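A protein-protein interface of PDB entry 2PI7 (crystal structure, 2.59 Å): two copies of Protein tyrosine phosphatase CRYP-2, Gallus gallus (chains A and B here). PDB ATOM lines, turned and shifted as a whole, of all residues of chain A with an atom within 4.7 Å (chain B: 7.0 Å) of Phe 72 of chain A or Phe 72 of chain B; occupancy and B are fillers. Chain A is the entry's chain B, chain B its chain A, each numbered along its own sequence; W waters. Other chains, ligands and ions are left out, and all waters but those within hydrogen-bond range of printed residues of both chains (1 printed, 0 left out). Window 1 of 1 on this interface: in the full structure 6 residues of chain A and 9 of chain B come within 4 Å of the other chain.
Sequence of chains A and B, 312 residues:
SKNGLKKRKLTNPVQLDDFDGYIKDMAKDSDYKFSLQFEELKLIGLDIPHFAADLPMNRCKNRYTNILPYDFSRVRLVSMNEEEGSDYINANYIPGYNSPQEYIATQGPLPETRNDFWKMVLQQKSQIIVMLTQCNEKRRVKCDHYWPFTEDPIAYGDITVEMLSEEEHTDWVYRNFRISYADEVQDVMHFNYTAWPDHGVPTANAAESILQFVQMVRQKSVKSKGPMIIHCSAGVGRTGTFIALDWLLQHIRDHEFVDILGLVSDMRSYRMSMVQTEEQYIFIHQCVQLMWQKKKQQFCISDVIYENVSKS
NH2 of Arg 76 of chain A sits at hydrogen-bond distance from OH of Tyr 270 of chain B (2.6 Å).
The side-chain hydroxyl (OG) of Ser 73 of chain A lies within hydrogen-bond range of the backbone carbonyl oxygen (O) of Tyr 270 of chain A, 2.6 Å away. The side-chain amide nitrogen (ND2) of Asn 92 of chain B sits at hydrogen-bond distance from the backbone carbonyl oxygen (O) of Tyr 270 of chain B (3.2 Å). The backbone carbonyl oxygen (O) of Pro 49 of chain B sits at hydrogen-bond distance from the backbone NH (N) of Asp 71 of chain B (3.0 Å). The side-chain hydroxyl (OG) of Ser 73 of chain B sits at hydrogen-bond distance from the backbone carbonyl oxygen (O) of Tyr 270 of chain B (2.5 Å). The backbone carbonyl oxygen (O) of Asp 71 of chain A lies within hydrogen-bond range of the guanidinium group (NH1) of Arg 76 of chain A, at 2.9 Å.
CD of Pro 49 of chain B touches CE2 of Phe 72 of chain A, at 3.4 Å. O of Phe 72 of chain A touches CB of Phe 72 of chain B, at 3.0 Å. CE2 of Phe 72 of chain B touches NH1 of Arg 76 of chain A (3.9 Å). Tyr 270 of chain A touches Pro 49 of chain B (OH to CB, 3.5 Å).
Printed residues of chain B within 4 Å of Phe 72 of chain A: Pro 49 (3.4 Å) and Phe 72 (3.0 Å). Arg 74 of chain A touches none of the printed residues of chain B. Printed residues of chain B within 4 Å of Arg 76 of chain A: Phe 72 and Tyr 270. Of the printed residues of chain B, Tyr 270 of chain A touches Pro 49 (3.5 Å). Printed residues of chain A within 4 Å of Pro 49 of chain B: Phe 72 and Tyr 270. Tyr 70 of chain B touches none of the printed residues of chain A. Of the printed residues of chain A, Tyr 270 of chain B touches Arg 76.
Hydrophobic or aromatic side chains of chain A within 4 Å of the printed part of chain B: Phe 72 and Tyr 270. Of the 18 printed residues of chain B, 3 touch a printed residue of chain A. Along chain B the printed residues that touch a printed residue of chain A span positions 49 to 270. Among the printed residues, 5 pairs touch across the chains. Among the printed residues, no Asp or Glu carboxylate lies within 4 Å of a Lys or Arg side-chain nitrogen of the other chain.
Phe 72 of chain A touches its own counterpart, Phe 72 of chain B. Arg 76 of chain A touches Phe 72 of chain B, but with the chains exchanged Phe 72 of chain A does not touch Arg 76 of chain B (9.2 Å). Arg 76 of chain A touches Tyr 270 of chain B, but with the chains exchanged Tyr 270 of chain A does not touch Arg 76 of chain B (9.4 Å).
Water W1 lies within hydrogen-bond range of the backbone carbonyl oxygen of Ser 269 of chain A (3.0 Å) and the backbone carbonyl oxygen of Asp 47 of chain B (3.4 Å).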
ATOM      1  N   ILE A  48      25.665  -2.419 -17.344  1.00  0.00           N
ATOM      2  CA  ILE A  48      25.334  -1.010 -17.172  1.00  0.00           C
ATOM      3  C   ILE A  48      24.668  -0.885 -15.815  1.00  0.00           C
ATOM      4  O   ILE A  48      23.651  -1.519 -15.546  1.00  0.00           O
ATOM      5  CB  ILE A  48      24.391  -0.522 -18.270  1.00  0.00           C
ATOM      6  CG1 ILE A  48      25.083  -0.642 -19.632  1.00  0.00           C
ATOM      7  CG2 ILE A  48      24.008   0.917 -18.009  1.00  0.00           C
ATOM      8  CD1 ILE A  48      24.234  -0.185 -20.818  1.00  0.00           C
ATOM      9  N   TYR A  70      18.340   1.171 -15.857  1.00  0.00           N
ATOM     10  CA  TYR A  70      19.719   1.636 -15.759  1.00  0.00           C
ATOM     11  C   TYR A  70      19.696   2.970 -15.007  1.00  0.00           C
ATOM     12  O   TYR A  70      18.685   3.671 -15.015  1.00  0.00           O
ATOM     13  CB  TYR A  70      20.319   1.829 -17.156  1.00  0.00           C
ATOM     14  CG  TYR A  70      20.373   0.567 -17.995  1.00  0.00           C
ATOM     15  CD1 TYR A  70      20.614  -0.677 -17.407  1.00  0.00           C
ATOM     16  CD2 TYR A  70      20.222   0.618 -19.387  1.00  0.00           C
ATOM     17  CE1 TYR A  70      20.699  -1.838 -18.176  1.00  0.00           C
ATOM     18  CE2 TYR A  70      20.311  -0.546 -20.172  1.00  0.00           C
ATOM     19  CZ  TYR A  70      20.547  -1.766 -19.551  1.00  0.00           C
ATOM     20  OH  TYR A  70      20.613  -2.920 -20.292  1.00  0.00           O
ATOM     21  N   ASP A  71      20.796   3.329 -14.355  1.00  0.00           N
ATOM     22  CA  ASP A  71      20.828   4.587 -13.620  1.00  0.00           C
ATOM     23  C   ASP A  71      20.784   5.831 -14.497  1.00  0.00           C
ATOM     24  O   ASP A  71      20.090   6.782 -14.175  1.00  0.00           O
ATOM     25  CB  ASP A  71      22.066   4.664 -12.722  1.00  0.00           C
ATOM     26  CG  ASP A  71      22.025   3.668 -11.577  1.00  0.00           C
ATOM     27  OD1 ASP A  71      20.997   3.605 -10.869  1.00  0.00           O
ATOM     28  OD2 ASP A  71      23.032   2.951 -11.376  1.00  0.00           O
ATOM     29  N   PHE A  72      21.507   5.835 -15.611  1.00  0.00           N
ATOM     30  CA  PHE A  72      21.532   7.029 -16.451  1.00  0.00           C
ATOM     31  C   PHE A  72      20.241   7.359 -17.189  1.00  0.00           C
ATOM     32  O   PHE A  72      19.822   8.525 -17.233  1.00  0.00           O
ATOM     33  CB  PHE A  72      22.690   6.966 -17.458  1.00  0.00           C
ATOM     34  CG  PHE A  72      22.392   6.165 -18.692  1.00  0.00           C
ATOM     35  CD1 PHE A  72      22.599   4.792 -18.716  1.00  0.00           C
ATOM     36  CD2 PHE A  72      21.923   6.792 -19.843  1.00  0.00           C
ATOM     37  CE1 PHE A  72      22.348   4.053 -19.871  1.00  0.00           C
ATOM     38  CE2 PHE A  72      21.667   6.059 -21.004  1.00  0.00           C
ATOM     39  CZ  PHE A  72      21.883   4.686 -21.015  1.00  0.00           C
ATOM     40  N   SER A  73      19.599   6.346 -17.755  1.00  0.00           N
ATOM     41  CA  SER A  73      18.377   6.569 -18.505  1.00  0.00           C
ATOM     42  C   SER A  73      17.092   6.491 -17.687  1.00  0.00           C
ATOM     43  O   SER A  73      16.002   6.619 -18.239  1.00  0.00           O
ATOM     44  CB  SER A  73      18.316   5.583 -19.680  1.00  0.00           C
ATOM     45  OG  SER A  73      18.501   4.249 -19.246  1.00  0.00           O
ATOM     46  N   ARG A  74      17.206   6.314 -16.373  1.00  0.00           N
ATOM     47  CA  ARG A  74      16.003   6.203 -15.558  1.00  0.00           C
ATOM     48  C   ARG A  74      15.225   7.490 -15.370  1.00  0.00           C
ATOM     49  O   ARG A  74      15.799   8.564 -15.246  1.00  0.00           O
ATOM     50  CB  ARG A  74      16.316   5.582 -14.189  1.00  0.00           C
ATOM     51  CG  ARG A  74      16.912   6.479 -13.123  1.00  0.00           C
ATOM     52  CD  ARG A  74      17.246   5.595 -11.930  1.00  0.00           C
ATOM     53  NE  ARG A  74      17.746   6.297 -10.752  1.00  0.00           N
ATOM     54  CZ  ARG A  74      17.008   7.046  -9.941  1.00  0.00           C
ATOM     55  NH1 ARG A  74      15.713   7.215 -10.163  1.00  0.00           N
ATOM     56  NH2 ARG A  74      17.568   7.624  -8.889  1.00  0.00           N
ATOM     57  N   ARG A  76      13.619   9.701 -13.150  1.00  0.00           N
ATOM     58  CA  ARG A  76      13.554   9.988 -11.724  1.00  0.00           C
ATOM     59  C   ARG A  76      12.432  10.976 -11.398  1.00  0.00           C
ATOM     60  O   ARG A  76      12.208  11.937 -12.128  1.00  0.00           O
ATOM     61  CB  ARG A  76      14.913  10.517 -11.222  1.00  0.00           C
ATOM     62  CG  ARG A  76      15.735  11.268 -12.261  1.00  0.00           C
ATOM     63  CD  ARG A  76      16.979  10.471 -12.703  1.00  0.00           C
ATOM     64  NE  ARG A  76      18.037  10.457 -11.691  1.00  0.00           N
ATOM     65  CZ  ARG A  76      19.252   9.949 -11.877  1.00  0.00           C
ATOM     66  NH1 ARG A  76      19.586   9.402 -13.035  1.00  0.00           N
ATOM     67  NH2 ARG A  76      20.145   9.994 -10.897  1.00  0.00           N
ATOM     68  N   SER A 269      20.445  -0.512 -24.958  1.00  0.00           N
ATOM     69  CA  SER A 269      21.467   0.263 -24.268  1.00  0.00           C
ATOM     70  C   SER A 269      20.784   1.228 -23.318  1.00  0.00           C
ATOM     71  O   SER A 269      21.426   1.822 -22.457  1.00  0.00           O
ATOM     72  CB  SER A 269      22.310   1.066 -25.260  1.00  0.00           C
ATOM     73  OG  SER A 269      23.169   0.227 -26.012  1.00  0.00           O
ATOM     74  N   TYR A 270      19.476   1.389 -23.483  1.00  0.00           N
ATOM     75  CA  TYR A 270      18.718   2.311 -22.649  1.00  0.00           C
ATOM     76  C   TYR A 270      17.857   1.621 -21.598  1.00  0.00           C
ATOM     77  O   TYR A 270      17.551   2.202 -20.558  1.00  0.00           O
ATOM     78  CB  TYR A 270      17.876   3.213 -23.547  1.00  0.00           C
ATOM     79  CG  TYR A 270      18.710   4.246 -24.275  1.00  0.00           C
ATOM     80  CD1 TYR A 270      18.839   5.550 -23.775  1.00  0.00           C
ATOM     81  CD2 TYR A 270      19.419   3.910 -25.422  1.00  0.00           C
ATOM     82  CE1 TYR A 270      19.654   6.487 -24.397  1.00  0.00           C
ATOM     83  CE2 TYR A 270      20.243   4.836 -26.047  1.00  0.00           C
ATOM     84  CZ  TYR A 270      20.356   6.121 -25.529  1.00  0.00           C
ATOM     85  OH  TYR A 270      21.189   7.031 -26.145  1.00  0.00           O
ATOM     86  N   ASP B  47      30.603   3.820 -20.497  1.00  0.00           N
ATOM     87  CA  ASP B  47      29.625   3.404 -21.494  1.00  0.00           C
ATOM     88  C   ASP B  47      28.271   4.109 -21.380  1.00  0.00           C
ATOM     89  O   ASP B  47      27.208   3.487 -21.472  1.00  0.00           O
ATOM     90  CB  ASP B  47      29.478   1.875 -21.445  1.00  0.00           C
ATOM     91  CG  ASP B  47      30.740   1.149 -21.955  1.00  0.00           C
ATOM     92  OD1 ASP B  47      30.872  -0.081 -21.751  1.00  0.00           O
ATOM     93  OD2 ASP B  47      31.607   1.817 -22.569  1.00  0.00           O
ATOM     94  N   ILE B  48      28.335   5.424 -21.196  1.00  0.00           N
ATOM     95  CA  ILE B  48      27.148   6.266 -21.082  1.00  0.00           C
ATOM     96  C   ILE B  48      27.056   7.177 -22.315  1.00  0.00           C
ATOM     97  O   ILE B  48      28.023   7.846 -22.688  1.00  0.00           O
ATOM     98  CB  ILE B  48      27.207   7.127 -19.798  1.00  0.00           C
ATOM     99  CG1 ILE B  48      27.095   6.226 -18.570  1.00  0.00           C
ATOM    100  CG2 ILE B  48      26.089   8.161 -19.804  1.00  0.00           C
ATOM    101  CD1 ILE B  48      27.117   6.980 -17.275  1.00  0.00           C
ATOM    102  N   PRO B  49      25.884   7.218 -22.961  1.00  0.00           N
ATOM    103  CA  PRO B  49      25.711   8.051 -24.153  1.00  0.00           C
ATOM    104  C   PRO B  49      25.986   9.538 -23.938  1.00  0.00           C
ATOM    105  O   PRO B  49      25.785  10.084 -22.843  1.00  0.00           O
ATOM    106  CB  PRO B  49      24.257   7.795 -24.549  1.00  0.00           C
ATOM    107  CG  PRO B  49      23.979   6.438 -23.984  1.00  0.00           C
ATOM    108  CD  PRO B  49      24.632   6.517 -22.636  1.00  0.00           C
ATOM    109  N   HIS B  50      26.460  10.175 -25.002  1.00  0.00           N
ATOM    110  CA  HIS B  50      26.743  11.598 -25.008  1.00  0.00           C
ATOM    111  C   HIS B  50      26.691  12.080 -26.452  1.00  0.00           C
ATOM    112  O   HIS B  50      27.557  12.830 -26.895  1.00  0.00           O
ATOM    113  CB  HIS B  50      28.113  11.894 -24.386  1.00  0.00           C
ATOM    114  CG  HIS B  50      29.259  11.191 -25.045  1.00  0.00           C
ATOM    115  ND1 HIS B  50      29.843  10.061 -24.512  1.00  0.00           N
ATOM    116  CD2 HIS B  50      29.952  11.478 -26.171  1.00  0.00           C
ATOM    117  CE1 HIS B  50      30.850   9.682 -25.280  1.00  0.00           C
ATOM    118  NE2 HIS B  50      30.937  10.526 -26.294  1.00  0.00           N
ATOM    119  N   PRO B  69      29.714  15.998 -22.112  1.00  0.00           N
ATOM    120  CA  PRO B  69      28.680  15.734 -21.109  1.00  0.00           C
ATOM    121  C   PRO B  69      27.819  14.529 -21.483  1.00  0.00           C
ATOM    122  O   PRO B  69      27.593  14.265 -22.661  1.00  0.00           O
ATOM    123  CB  PRO B  69      27.875  17.031 -21.109  1.00  0.00           C
ATOM    124  CG  PRO B  69      27.895  17.409 -22.573  1.00  0.00           C
ATOM    125  CD  PRO B  69      29.349  17.155 -22.955  1.00  0.00           C
ATOM    126  N   TYR B  70      27.350  13.793 -20.482  1.00  0.00           N
ATOM    127  CA  TYR B  70      26.481  12.645 -20.728  1.00  0.00           C
ATOM    128  C   TYR B  70      25.126  13.237 -21.094  1.00  0.00           C
ATOM    129  O   TYR B  70      24.739  14.242 -20.521  1.00  0.00           O
ATOM    130  CB  TYR B  70      26.311  11.796 -19.459  1.00  0.00           C
ATOM    131  CG  TYR B  70      27.586  11.223 -18.889  1.00  0.00           C
ATOM    132  CD1 TYR B  70      28.491  10.542 -19.699  1.00  0.00           C
ATOM    133  CD2 TYR B  70      27.878  11.343 -17.532  1.00  0.00           C
ATOM    134  CE1 TYR B  70      29.663   9.991 -19.172  1.00  0.00           C
ATOM    135  CE2 TYR B  70      29.037  10.801 -16.991  1.00  0.00           C
ATOM    136  CZ  TYR B  70      29.931  10.123 -17.819  1.00  0.00           C
ATOM    137  OH  TYR B  70      31.091   9.584 -17.295  1.00  0.00           O
ATOM    138  N   ASP B  71      24.405  12.625 -22.030  1.00  0.00           N
ATOM    139  CA  ASP B  71      23.087  13.136 -22.412  1.00  0.00           C
ATOM    140  C   ASP B  71      22.142  13.287 -21.226  1.00  0.00           C
ATOM    141  O   ASP B  71      21.571  14.349 -21.001  1.00  0.00           O
ATOM    142  CB  ASP B  71      22.368  12.207 -23.400  1.00  0.00           C
ATOM    143  CG  ASP B  71      23.060  12.095 -24.727  1.00  0.00           C
ATOM    144  OD1 ASP B  71      23.756  13.055 -25.125  1.00  0.00           O
ATOM    145  OD2 ASP B  71      22.883  11.039 -25.382  1.00  0.00           O
ATOM    146  N   PHE B  72      21.968  12.205 -20.477  1.00  0.00           N
ATOM    147  CA  PHE B  72      21.031  12.213 -19.364  1.00  0.00           C
ATOM    148  C   PHE B  72      21.126  13.383 -18.400  1.00  0.00           C
ATOM    149  O   PHE B  72      20.104  13.961 -18.027  1.00  0.00           O
ATOM    150  CB  PHE B  72      21.110  10.900 -18.581  1.00  0.00           C
ATOM    151  CG  PHE B  72      22.022  10.943 -17.392  1.00  0.00           C
ATOM    152  CD1 PHE B  72      23.381  10.648 -17.522  1.00  0.00           C
ATOM    153  CD2 PHE B  72      21.517  11.251 -16.132  1.00  0.00           C
ATOM    154  CE1 PHE B  72      24.223  10.658 -16.405  1.00  0.00           C
ATOM    155  CE2 PHE B  72      22.334  11.265 -15.022  1.00  0.00           C
ATOM    156  CZ  PHE B  72      23.695  10.967 -15.152  1.00  0.00           C
ATOM    157  N   SER B  73      22.342  13.749 -18.015  1.00  0.00           N
ATOM    158  CA  SER B  73      22.525  14.827 -17.051  1.00  0.00           C
ATOM    159  C   SER B  73      22.945  16.179 -17.608  1.00  0.00           C
ATOM    160  O   SER B  73      23.109  17.126 -16.832  1.00  0.00           O
ATOM    161  CB  SER B  73      23.539  14.401 -15.990  1.00  0.00           C
ATOM    162  OG  SER B  73      24.837  14.267 -16.552  1.00  0.00           O
ATOM    163  N   ARG B  74      23.104  16.302 -18.926  1.00  0.00           N
ATOM    164  CA  ARG B  74      23.534  17.588 -19.457  1.00  0.00           C
ATOM    165  C   ARG B  74      22.554  18.712 -19.186  1.00  0.00           C
ATOM    166  O   ARG B  74      21.380  18.470 -18.915  1.00  0.00           O
ATOM    167  CB  ARG B  74      23.848  17.497 -20.957  1.00  0.00           C
ATOM    168  CG  ARG B  74      22.696  17.517 -21.920  1.00  0.00           C
ATOM    169  CD  ARG B  74      23.263  17.378 -23.329  1.00  0.00           C
ATOM    170  NE  ARG B  74      22.242  17.216 -24.366  1.00  0.00           N
ATOM    171  CZ  ARG B  74      21.606  18.215 -24.972  1.00  0.00           C
ATOM    172  NH1 ARG B  74      21.875  19.476 -24.659  1.00  0.00           N
ATOM    173  NH2 ARG B  74      20.696  17.949 -25.898  1.00  0.00           N
ATOM    174  N   VAL B  75      23.053  19.946 -19.211  1.00  0.00           N
ATOM    175  CA  VAL B  75      22.212  21.123 -18.977  1.00  0.00           C
ATOM    176  C   VAL B  75      21.776  21.650 -20.340  1.00  0.00           C
ATOM    177  O   VAL B  75      22.607  21.877 -21.219  1.00  0.00           O
ATOM    178  CB  VAL B  75      22.966  22.266 -18.242  1.00  0.00           C
ATOM    179  CG1 VAL B  75      21.989  23.359 -17.869  1.00  0.00           C
ATOM    180  CG2 VAL B  75      23.649  21.746 -17.010  1.00  0.00           C
ATOM    181  N   ARG B  76      20.475  21.845 -20.509  1.00  0.00           N
ATOM    182  CA  ARG B  76      19.958  22.323 -21.780  1.00  0.00           C
ATOM    183  C   ARG B  76      19.573  23.799 -21.791  1.00  0.00           C
ATOM    184  O   ARG B  76      18.955  24.315 -20.856  1.00  0.00           O
ATOM    185  CB  ARG B  76      18.743  21.492 -22.210  1.00  0.00           C
ATOM    186  CG  ARG B  76      19.020  20.017 -22.439  1.00  0.00           C
ATOM    187  CD  ARG B  76      17.778  19.309 -22.971  1.00  0.00           C
ATOM    188  NE  ARG B  76      18.012  17.900 -23.289  1.00  0.00           N
ATOM    189  CZ  ARG B  76      18.452  16.994 -22.417  1.00  0.00           C
ATOM    190  NH1 ARG B  76      18.632  15.733 -22.795  1.00  0.00           N
ATOM    191  NH2 ARG B  76      18.716  17.351 -21.165  1.00  0.00           N
ATOM    192  N   ASN B  92      26.940  19.620 -17.010  1.00  0.00           N
ATOM    193  CA  ASN B  92      26.160  18.544 -16.390  1.00  0.00           C
ATOM    194  C   ASN B  92      25.701  18.904 -14.980  1.00  0.00           C
ATOM    195  O   ASN B  92      26.430  19.558 -14.232  1.00  0.00           O
ATOM    196  CB  ASN B  92      26.975  17.248 -16.286  1.00  0.00           C
ATOM    197  CG  ASN B  92      27.365  16.690 -17.631  1.00  0.00           C
ATOM    198  OD1 ASN B  92      28.472  16.931 -18.118  1.00  0.00           O
ATOM    199  ND2 ASN B  92      26.454  15.940 -18.249  1.00  0.00           N
ATOM    200  N   TYR B  93      24.491  18.478 -14.623  1.00  0.00           N
ATOM    201  CA  TYR B  93      23.966  18.710 -13.284  1.00  0.00           C
ATOM    202  C   TYR B  93      24.732  17.704 -12.432  1.00  0.00           C
ATOM    203  O   TYR B  93      24.995  16.597 -12.882  1.00  0.00           O
ATOM    204  CB  TYR B  93      22.463  18.386 -13.228  1.00  0.00           C
ATOM    205  CG  TYR B  93      21.563  19.382 -13.937  1.00  0.00           C
ATOM    206  CD1 TYR B  93      21.309  20.637 -13.387  1.00  0.00           C
ATOM    207  CD2 TYR B  93      20.987  19.082 -15.170  1.00  0.00           C
ATOM    208  CE1 TYR B  93      20.509  21.569 -14.047  1.00  0.00           C
ATOM    209  CE2 TYR B  93      20.177  20.010 -15.842  1.00  0.00           C
ATOM    210  CZ  TYR B  93      19.944  21.250 -15.277  1.00  0.00           C
ATOM    211  OH  TYR B  93      19.155  22.183 -15.929  1.00  0.00           O
ATOM    212  N   GLN B 101      21.199  17.926  -8.713  1.00  0.00           N
ATOM    213  CA  GLN B 101      21.316  19.119  -9.542  1.00  0.00           C
ATOM    214  C   GLN B 101      21.629  20.353  -8.689  1.00  0.00           C
ATOM    215  O   GLN B 101      21.262  21.475  -9.037  1.00  0.00           O
ATOM    216  CB  GLN B 101      20.020  19.328 -10.335  1.00  0.00           C
ATOM    217  CG  GLN B 101      19.532  18.044 -11.008  1.00  0.00           C
ATOM    218  CD  GLN B 101      18.335  18.260 -11.904  1.00  0.00           C
ATOM    219  OE1 GLN B 101      17.400  18.977 -11.541  1.00  0.00           O
ATOM    220  NE2 GLN B 101      18.344  17.626 -13.080  1.00  0.00           N
ATOM    221  N   SER B 269      29.438   9.652 -12.450  1.00  0.00           N
ATOM    222  CA  SER B 269      28.384   9.037 -13.259  1.00  0.00           C
ATOM    223  C   SER B 269      27.447  10.111 -13.822  1.00  0.00           C
ATOM    224  O   SER B 269      26.527   9.805 -14.575  1.00  0.00           O
ATOM    225  CB  SER B 269      27.583   8.031 -12.442  1.00  0.00           C
ATOM    226  OG  SER B 269      26.820   8.694 -11.458  1.00  0.00           O
ATOM    227  N   TYR B 270      27.709  11.368 -13.456  1.00  0.00           N
ATOM    228  CA  TYR B 270      26.928  12.520 -13.908  1.00  0.00           C
ATOM    229  C   TYR B 270      27.737  13.344 -14.914  1.00  0.00           C
ATOM    230  O   TYR B 270      27.173  14.080 -15.729  1.00  0.00           O
ATOM    231  CB  TYR B 270      26.509  13.372 -12.701  1.00  0.00           C
ATOM    232  CG  TYR B 270      25.418  12.708 -11.887  1.00  0.00           C
ATOM    233  CD1 TYR B 270      24.069  12.854 -12.237  1.00  0.00           C
ATOM    234  CD2 TYR B 270      25.733  11.864 -10.822  1.00  0.00           C
ATOM    235  CE1 TYR B 270      23.066  12.175 -11.552  1.00  0.00           C
ATOM    236  CE2 TYR B 270      24.738  11.175 -10.133  1.00  0.00           C
ATOM    237  CZ  TYR B 270      23.406  11.332 -10.504  1.00  0.00           C
ATOM    238  OH  TYR B 270      22.430  10.617  -9.842  1.00  0.00           O
ATOM    239  N   ARG B 271      29.058  13.205 -14.842  1.00  0.00           N
ATOM    240  CA  ARG B 271      29.989  13.881 -15.754  1.00  0.00           C
ATOM    241  C   ARG B 271      31.318  13.133 -15.666  1.00  0.00           C
ATOM    242  O   ARG B 271      31.763  12.758 -14.575  1.00  0.00           O
ATOM    243  CB  ARG B 271      30.204  15.353 -15.383  1.00  0.00           C
ATOM    244  CG  ARG B 271      31.099  16.119 -16.371  1.00  0.00           C
ATOM    245  CD  ARG B 271      31.323  17.573 -15.908  1.00  0.00           C
ATOM    246  NE  ARG B 271      32.233  18.378 -16.737  1.00  0.00           N
ATOM    247  CZ  ARG B 271      31.962  18.825 -17.963  1.00  0.00           C
ATOM    248  NH1 ARG B 271      30.807  18.547 -18.543  1.00  0.00           N
ATOM    249  NH2 ARG B 271      32.837  19.585 -18.603  1.00  0.00           N
HETATM  250  O   HOH W   1      24.254   2.734 -23.057  1.00  0.00           O
